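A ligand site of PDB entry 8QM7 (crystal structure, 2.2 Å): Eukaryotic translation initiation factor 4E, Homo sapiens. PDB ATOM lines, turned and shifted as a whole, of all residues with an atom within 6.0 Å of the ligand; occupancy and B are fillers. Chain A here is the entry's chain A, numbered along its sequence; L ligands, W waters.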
ATOM      1  N   LEU A  43      -0.388 -22.402 -24.578  1.00  0.00           N
ATOM      2  CA  LEU A  43       0.402 -21.229 -24.356  1.00  0.00           C
ATOM      3  C   LEU A  43       1.136 -20.872 -25.622  1.00  0.00           C
ATOM      4  O   LEU A  43       1.834 -21.712 -26.179  1.00  0.00           O
ATOM      5  CB  LEU A  43       1.408 -21.469 -23.215  1.00  0.00           C
ATOM      6  CG  LEU A  43       2.392 -20.315 -22.950  1.00  0.00           C
ATOM      7  CD1 LEU A  43       1.654 -19.037 -22.578  1.00  0.00           C
ATOM      8  CD2 LEU A  43       3.429 -20.742 -21.924  1.00  0.00           C
ATOM      9  N   PHE A  64      -1.538 -28.126 -22.008  1.00  0.00           N
ATOM     10  CA  PHE A  64      -1.748 -28.759 -20.700  1.00  0.00           C
ATOM     11  C   PHE A  64      -3.219 -28.862 -20.396  1.00  0.00           C
ATOM     12  O   PHE A  64      -4.008 -28.098 -20.901  1.00  0.00           O
ATOM     13  CB  PHE A  64      -0.979 -28.056 -19.559  1.00  0.00           C
ATOM     14  CG  PHE A  64      -1.397 -26.603 -19.317  1.00  0.00           C
ATOM     15  CD1 PHE A  64      -2.480 -26.304 -18.502  1.00  0.00           C
ATOM     16  CD2 PHE A  64      -0.749 -25.575 -19.960  1.00  0.00           C
ATOM     17  CE1 PHE A  64      -2.902 -24.987 -18.343  1.00  0.00           C
ATOM     18  CE2 PHE A  64      -1.164 -24.257 -19.780  1.00  0.00           C
ATOM     19  CZ  PHE A  64      -2.247 -23.979 -18.978  1.00  0.00           C
ATOM     20  N   PHE A  70      -0.126 -27.279 -15.453  1.00  0.00           N
ATOM     21  CA  PHE A  70      -0.158 -25.807 -15.469  1.00  0.00           C
ATOM     22  C   PHE A  70       0.940 -25.267 -14.577  1.00  0.00           C
ATOM     23  O   PHE A  70       1.725 -24.451 -15.019  1.00  0.00           O
ATOM     24  CB  PHE A  70      -1.536 -25.254 -15.015  1.00  0.00           C
ATOM     25  CG  PHE A  70      -1.436 -23.807 -14.595  1.00  0.00           C
ATOM     26  CD1 PHE A  70      -1.318 -22.803 -15.548  1.00  0.00           C
ATOM     27  CD2 PHE A  70      -1.416 -23.454 -13.251  1.00  0.00           C
ATOM     28  CE1 PHE A  70      -1.220 -21.477 -15.141  1.00  0.00           C
ATOM     29  CE2 PHE A  70      -1.312 -22.129 -12.865  1.00  0.00           C
ATOM     30  CZ  PHE A  70      -1.192 -21.154 -13.802  1.00  0.00           C
ATOM     31  N   LEU A  73       4.577 -25.811 -15.899  1.00  0.00           N
ATOM     32  CA  LEU A  73       4.862 -24.859 -16.983  1.00  0.00           C
ATOM     33  C   LEU A  73       5.027 -23.479 -16.419  1.00  0.00           C
ATOM     34  O   LEU A  73       5.959 -22.764 -16.816  1.00  0.00           O
ATOM     35  CB  LEU A  73       3.709 -24.898 -18.007  1.00  0.00           C
ATOM     36  CG  LEU A  73       3.806 -23.920 -19.171  1.00  0.00           C
ATOM     37  CD1 LEU A  73       5.023 -24.225 -20.013  1.00  0.00           C
ATOM     38  CD2 LEU A  73       2.555 -23.981 -20.013  1.00  0.00           C
ATOM     39  N   TYR A  74       4.150 -23.073 -15.484  1.00  0.00           N
ATOM     40  CA  TYR A  74       4.244 -21.771 -14.847  1.00  0.00           C
ATOM     41  C   TYR A  74       5.583 -21.595 -14.131  1.00  0.00           C
ATOM     42  O   TYR A  74       6.278 -20.585 -14.334  1.00  0.00           O
ATOM     43  CB  TYR A  74       3.079 -21.574 -13.859  1.00  0.00           C
ATOM     44  CG  TYR A  74       3.062 -20.190 -13.259  1.00  0.00           C
ATOM     45  CD1 TYR A  74       3.779 -19.909 -12.086  1.00  0.00           C
ATOM     46  CD2 TYR A  74       2.317 -19.157 -13.827  1.00  0.00           C
ATOM     47  CE1 TYR A  74       3.778 -18.638 -11.536  1.00  0.00           C
ATOM     48  CE2 TYR A  74       2.295 -17.897 -13.283  1.00  0.00           C
ATOM     49  CZ  TYR A  74       3.033 -17.637 -12.130  1.00  0.00           C
ATOM     50  OH  TYR A  74       3.033 -16.386 -11.593  1.00  0.00           O
ATOM     51  N   ILE A  77       8.464 -21.364 -16.868  1.00  0.00           N
ATOM     52  CA  ILE A  77       8.534 -20.028 -17.481  1.00  0.00           C
ATOM     53  C   ILE A  77       9.058 -18.983 -16.453  1.00  0.00           C
ATOM     54  O   ILE A  77       9.911 -18.175 -16.776  1.00  0.00           O
ATOM     55  CB  ILE A  77       7.126 -19.574 -18.019  1.00  0.00           C
ATOM     56  CG1 ILE A  77       6.571 -20.488 -19.161  1.00  0.00           C
ATOM     57  CG2 ILE A  77       7.183 -18.127 -18.469  1.00  0.00           C
ATOM     58  CD1 ILE A  77       7.234 -20.295 -20.583  1.00  0.00           C
ATOM     59  N   GLN A  78       8.529 -19.013 -15.225  1.00  0.00           N
ATOM     60  CA  GLN A  78       8.859 -18.054 -14.169  1.00  0.00           C
ATOM     61  C   GLN A  78      10.374 -18.077 -13.857  1.00  0.00           C
ATOM     62  O   GLN A  78      10.945 -17.021 -13.590  1.00  0.00           O
ATOM     63  CB  GLN A  78       8.061 -18.373 -12.882  1.00  0.00           C
ATOM     64  CG  GLN A  78       7.856 -17.212 -11.905  1.00  0.00           C
ATOM     65  CD  GLN A  78       7.212 -17.652 -10.594  1.00  0.00           C
ATOM     66  OE1 GLN A  78       7.255 -18.827 -10.195  1.00  0.00           O
ATOM     67  NE2 GLN A  78       6.573 -16.730  -9.903  1.00  0.00           N
ATOM     68  N   LEU A  79      11.015 -19.256 -13.899  1.00  0.00           N
ATOM     69  CA  LEU A  79      12.461 -19.399 -13.675  1.00  0.00           C
ATOM     70  C   LEU A  79      13.325 -19.288 -14.950  1.00  0.00           C
ATOM     71  O   LEU A  79      14.442 -18.802 -14.870  1.00  0.00           O
ATOM     72  CB  LEU A  79      12.756 -20.723 -12.970  1.00  0.00           C
ATOM     73  CG  LEU A  79      12.013 -20.966 -11.648  1.00  0.00           C
ATOM     74  CD1 LEU A  79      11.959 -22.452 -11.330  1.00  0.00           C
ATOM     75  CD2 LEU A  79      12.651 -20.137 -10.481  1.00  0.00           C
ATOM     76  N   SER A  81      12.567 -17.661 -17.999  1.00  0.00           N
ATOM     77  CA  SER A  81      12.244 -16.628 -18.980  1.00  0.00           C
ATOM     78  C   SER A  81      12.398 -15.266 -18.372  1.00  0.00           C
ATOM     79  O   SER A  81      12.092 -15.089 -17.188  1.00  0.00           O
ATOM     80  CB  SER A  81      10.819 -16.807 -19.516  1.00  0.00           C
ATOM     81  OG  SER A  81      10.617 -18.053 -20.160  1.00  0.00           O
ATOM     82  N   ASN A  82      12.870 -14.308 -19.187  1.00  0.00           N
ATOM     83  CA  ASN A  82      12.992 -12.902 -18.800  1.00  0.00           C
ATOM     84  C   ASN A  82      12.071 -12.028 -19.677  1.00  0.00           C
ATOM     85  O   ASN A  82      11.735 -12.400 -20.808  1.00  0.00           O
ATOM     86  CB  ASN A  82      14.455 -12.404 -18.905  1.00  0.00           C
ATOM     87  CG  ASN A  82      15.260 -12.432 -17.614  1.00  0.00           C
ATOM     88  OD1 ASN A  82      14.813 -12.890 -16.544  1.00  0.00           O
ATOM     89  ND2 ASN A  82      16.490 -11.932 -17.689  1.00  0.00           N
ATOM     90  N   LEU A  83      11.705 -10.864 -19.148  1.00  0.00           N
ATOM     91  CA  LEU A  83      10.656 -10.026 -19.719  1.00  0.00           C
ATOM     92  C   LEU A  83      11.182  -9.106 -20.839  1.00  0.00           C
ATOM     93  O   LEU A  83      12.014  -8.230 -20.584  1.00  0.00           O
ATOM     94  CB  LEU A  83      10.060  -9.191 -18.577  1.00  0.00           C
ATOM     95  CG  LEU A  83       8.811  -8.405 -18.895  1.00  0.00           C
ATOM     96  CD1 LEU A  83       7.609  -9.321 -19.069  1.00  0.00           C
ATOM     97  CD2 LEU A  83       8.568  -7.408 -17.799  1.00  0.00           C
ATOM     98  N   MET A  84      10.664  -9.292 -22.075  1.00  0.00           N
ATOM     99  CA  MET A  84      11.080  -8.532 -23.265  1.00  0.00           C
ATOM    100  C   MET A  84       9.886  -7.757 -23.791  1.00  0.00           C
ATOM    101  O   MET A  84       8.899  -8.396 -24.155  1.00  0.00           O
ATOM    102  CB  MET A  84      11.526  -9.492 -24.393  1.00  0.00           C
ATOM    103  CG  MET A  84      12.960  -9.994 -24.278  1.00  0.00           C
ATOM    104  SD  MET A  84      13.391 -11.150 -25.619  1.00  0.00           S
ATOM    105  CE  MET A  84      12.247 -12.588 -25.234  1.00  0.00           C
ATOM    106  N   TYR A  89       2.376 -12.938 -24.668  1.00  0.00           N
ATOM    107  CA  TYR A  89       1.985 -14.284 -24.297  1.00  0.00           C
ATOM    108  C   TYR A  89       0.467 -14.379 -24.282  1.00  0.00           C
ATOM    109  O   TYR A  89      -0.231 -13.412 -23.932  1.00  0.00           O
ATOM    110  CB  TYR A  89       2.545 -14.648 -22.924  1.00  0.00           C
ATOM    111  CG  TYR A  89       4.055 -14.811 -22.885  1.00  0.00           C
ATOM    112  CD1 TYR A  89       4.886 -13.715 -22.788  1.00  0.00           C
ATOM    113  CD2 TYR A  89       4.629 -16.072 -22.919  1.00  0.00           C
ATOM    114  CE1 TYR A  89       6.268 -13.872 -22.745  1.00  0.00           C
ATOM    115  CE2 TYR A  89       6.005 -16.240 -22.868  1.00  0.00           C
ATOM    116  CZ  TYR A  89       6.828 -15.134 -22.764  1.00  0.00           C
ATOM    117  OH  TYR A  89       8.197 -15.280 -22.693  1.00  0.00           O
ATOM    118  N   SER A  90      -0.048 -15.521 -24.672  1.00  0.00           N
ATOM    119  CA  SER A  90      -1.478 -15.800 -24.761  1.00  0.00           C
ATOM    120  C   SER A  90      -1.713 -17.213 -24.285  1.00  0.00           C
ATOM    121  O   SER A  90      -1.000 -18.114 -24.718  1.00  0.00           O
ATOM    122  CB  SER A  90      -1.958 -15.738 -26.201  1.00  0.00           C
ATOM    123  OG  SER A  90      -1.750 -14.463 -26.766  1.00  0.00           O
ATOM    124  N   LEU A  91      -2.709 -17.416 -23.388  1.00  0.00           N
ATOM    125  CA  LEU A  91      -3.232 -18.712 -23.087  1.00  0.00           C
ATOM    126  C   LEU A  91      -4.610 -18.841 -23.663  1.00  0.00           C
ATOM    127  O   LEU A  91      -5.491 -18.146 -23.203  1.00  0.00           O
ATOM    128  CB  LEU A  91      -3.274 -18.964 -21.592  1.00  0.00           C
ATOM    129  CG  LEU A  91      -3.637 -20.416 -21.179  1.00  0.00           C
ATOM    130  CD1 LEU A  91      -2.440 -21.364 -21.422  1.00  0.00           C
ATOM    131  CD2 LEU A  91      -4.084 -20.508 -19.737  1.00  0.00           C
ATOM    132  N   LEU A 124       2.116  -6.642 -12.888  1.00  0.00           N
ATOM    133  CA  LEU A 124       2.080  -7.487 -14.083  1.00  0.00           C
ATOM    134  C   LEU A 124       2.007  -8.970 -13.715  1.00  0.00           C
ATOM    135  O   LEU A 124       1.096  -9.641 -14.144  1.00  0.00           O
ATOM    136  CB  LEU A 124       3.295  -7.232 -14.942  1.00  0.00           C
ATOM    137  CG  LEU A 124       3.383  -7.983 -16.312  1.00  0.00           C
ATOM    138  CD1 LEU A 124       2.225  -7.614 -17.229  1.00  0.00           C
ATOM    139  CD2 LEU A 124       4.699  -7.654 -17.038  1.00  0.00           C
ATOM    140  N   ASN A 125       2.940  -9.497 -12.905  1.00  0.00           N
ATOM    141  CA  ASN A 125       2.988 -10.910 -12.618  1.00  0.00           C
ATOM    142  C   ASN A 125       1.778 -11.339 -11.804  1.00  0.00           C
ATOM    143  O   ASN A 125       1.184 -12.346 -12.080  1.00  0.00           O
ATOM    144  CB  ASN A 125       4.291 -11.269 -11.947  1.00  0.00           C
ATOM    145  CG  ASN A 125       5.477 -11.060 -12.873  1.00  0.00           C
ATOM    146  OD1 ASN A 125       5.449 -11.402 -14.047  1.00  0.00           O
ATOM    147  ND2 ASN A 125       6.543 -10.500 -12.392  1.00  0.00           N
ATOM    148  N   TRP A 128      -1.460 -11.149 -14.041  1.00  0.00           N
ATOM    149  CA  TRP A 128      -1.417 -12.169 -15.049  1.00  0.00           C
ATOM    150  C   TRP A 128      -1.705 -13.546 -14.460  1.00  0.00           C
ATOM    151  O   TRP A 128      -2.500 -14.282 -15.038  1.00  0.00           O
ATOM    152  CB  TRP A 128      -0.044 -12.157 -15.756  1.00  0.00           C
ATOM    153  CG  TRP A 128       0.087 -13.189 -16.845  1.00  0.00           C
ATOM    154  CD1 TRP A 128       1.056 -14.137 -16.958  1.00  0.00           C
ATOM    155  CD2 TRP A 128      -0.747 -13.333 -17.995  1.00  0.00           C
ATOM    156  NE1 TRP A 128       0.903 -14.845 -18.116  1.00  0.00           N
ATOM    157  CE2 TRP A 128      -0.199 -14.376 -18.780  1.00  0.00           C
ATOM    158  CE3 TRP A 128      -1.885 -12.652 -18.467  1.00  0.00           C
ATOM    159  CZ2 TRP A 128      -0.777 -14.783 -19.971  1.00  0.00           C
ATOM    160  CZ3 TRP A 128      -2.475 -13.087 -19.627  1.00  0.00           C
ATOM    161  CH2 TRP A 128      -1.912 -14.107 -20.386  1.00  0.00           C
ATOM    162  N   LEU A 132      -4.783 -16.097 -15.343  1.00  0.00           N
ATOM    163  CA  LEU A 132      -4.561 -17.502 -15.643  1.00  0.00           C
ATOM    164  C   LEU A 132      -5.430 -18.414 -14.774  1.00  0.00           C
ATOM    165  O   LEU A 132      -6.023 -19.348 -15.296  1.00  0.00           O
ATOM    166  CB  LEU A 132      -3.087 -17.867 -15.455  1.00  0.00           C
ATOM    167  CG  LEU A 132      -2.076 -17.173 -16.365  1.00  0.00           C
ATOM    168  CD1 LEU A 132      -0.677 -17.621 -16.040  1.00  0.00           C
ATOM    169  CD2 LEU A 132      -2.390 -17.355 -17.822  1.00  0.00           C
ATOM    170  N   VAL A 152      -1.352 -11.113 -22.744  1.00  0.00           N
ATOM    171  CA  VAL A 152      -0.539 -10.103 -22.129  1.00  0.00           C
ATOM    172  C   VAL A 152       0.370  -9.515 -23.212  1.00  0.00           C
ATOM    173  O   VAL A 152       1.139 -10.214 -23.802  1.00  0.00           O
ATOM    174  CB  VAL A 152       0.205 -10.555 -20.842  1.00  0.00           C
ATOM    175  CG1 VAL A 152       1.094 -11.767 -21.090  1.00  0.00           C
ATOM    176  CG2 VAL A 152       1.025  -9.408 -20.279  1.00  0.00           C
ATOM    177  N   VAL A 154       3.403  -7.056 -23.513  1.00  0.00           N
ATOM    178  CA  VAL A 154       4.482  -6.388 -22.778  1.00  0.00           C
ATOM    179  C   VAL A 154       4.974  -5.252 -23.649  1.00  0.00           C
ATOM    180  O   VAL A 154       5.435  -5.518 -24.769  1.00  0.00           O
ATOM    181  CB  VAL A 154       5.613  -7.380 -22.454  1.00  0.00           C
ATOM    182  CG1 VAL A 154       6.710  -6.716 -21.649  1.00  0.00           C
ATOM    183  CG2 VAL A 154       5.055  -8.566 -21.684  1.00  0.00           C
HETATM  184  C1  LIG L   1       4.047 -11.632 -18.907  1.00  0.00           C
HETATM  185  C2  LIG L   1       4.526 -12.605 -17.879  1.00  0.00           C
HETATM  186  C3  LIG L   1       5.412 -13.718 -18.445  1.00  0.00           C
HETATM  187  C4  LIG L   1       7.679 -14.640 -17.958  1.00  0.00           C
HETATM  188  C5  LIG L   1       8.453 -14.972 -16.687  1.00  0.00           C
HETATM  189  C6  LIG L   1       8.543 -13.929 -18.976  1.00  0.00           C
HETATM  190  C7  LIG L   1       4.234 -15.596 -19.646  1.00  0.00           C
HETATM  191  C8  LIG L   1       3.516 -16.783 -19.678  1.00  0.00           C
HETATM  192  C9  LIG L   1       3.260 -17.488 -18.519  1.00  0.00           C
HETATM  193  C10 LIG L   1       3.669 -16.927 -17.311  1.00  0.00           C
HETATM  194  C11 LIG L   1       4.374 -15.739 -17.251  1.00  0.00           C
HETATM  195  C12 LIG L   1       4.515 -15.805 -14.762  1.00  0.00           C
HETATM  196  C13 LIG L   1       2.433 -18.727 -18.501  1.00  0.00           C
HETATM  197  C14 LIG L   1       2.089 -20.954 -17.680  1.00  0.00           C
HETATM  198  C15 LIG L   1       0.834 -20.999 -18.282  1.00  0.00           C
HETATM  199  C16 LIG L   1       0.386 -19.901 -18.972  1.00  0.00           C
HETATM  200  C17 LIG L   1       1.172 -18.780 -19.066  1.00  0.00           C
HETATM  201  O1  LIG L   1       6.593 -13.732 -17.624  1.00  0.00           O
HETATM  202  O2  LIG L   1       8.768 -12.597 -18.560  1.00  0.00           O
HETATM  203  C18 LIG L   1       4.673 -15.054 -18.438  1.00  0.00           C
HETATM  204  N1  LIG L   1       4.785 -15.219 -16.054  1.00  0.00           N
HETATM  205  C19 LIG L   1       5.094 -14.981 -13.635  1.00  0.00           C
HETATM  206  O3  LIG L   1       6.426 -14.583 -13.941  1.00  0.00           O
HETATM  207  C20 LIG L   1       2.861 -19.823 -17.774  1.00  0.00           C
HETATM  208  F1  LIG L   1       0.717 -17.724 -19.774  1.00  0.00           F
HETATM  209  O   HOH W   1       7.242 -11.432 -15.780  1.00  0.00           O
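N of Leu 83 sits close to O2 of the ligand. O3 of the ligand is in hydrogen-bond range of OD1 of Asn 125 (3.3 Å).
O of Tyr 89 sits at hydrogen-bond distance from N of Val 152, at 2.8 Å. O of Ile 77 lies close to OG of Ser 81 (3.5 Å).
NE1 of Trp 128 sits close to F1 of the ligand, at 3.3 Å. Residues that only touch the ligand: Leu 43, Phe 70, Leu 73, Tyr 74, Ile 77, Gln 78, Ser 81, Asn 82, Tyr 89, Leu 132 and Val 152. Hydrophobic or aromatic side chains that line the ligand: Leu 43, Phe 70, Leu 73, Tyr 74, Ile 77, Leu 83, Tyr 89, Trp 128, Leu 132 and Val 152. Within 4 Å of the ligand: Leu 43, Phe 70, Leu 73, Tyr 74, Ile 77, Gln 78, Ser 81, Asn 82, Leu 83, Tyr 89, Asn 125, Trp 128, Leu 132 and Val 152. The nearest printed residue that does not touch the ligand is Leu 91 (4.02 Å).
Water W1 bridges OD1 of Asn 125 (2.5 Å) and O1 of the ligand (3.0 Å).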
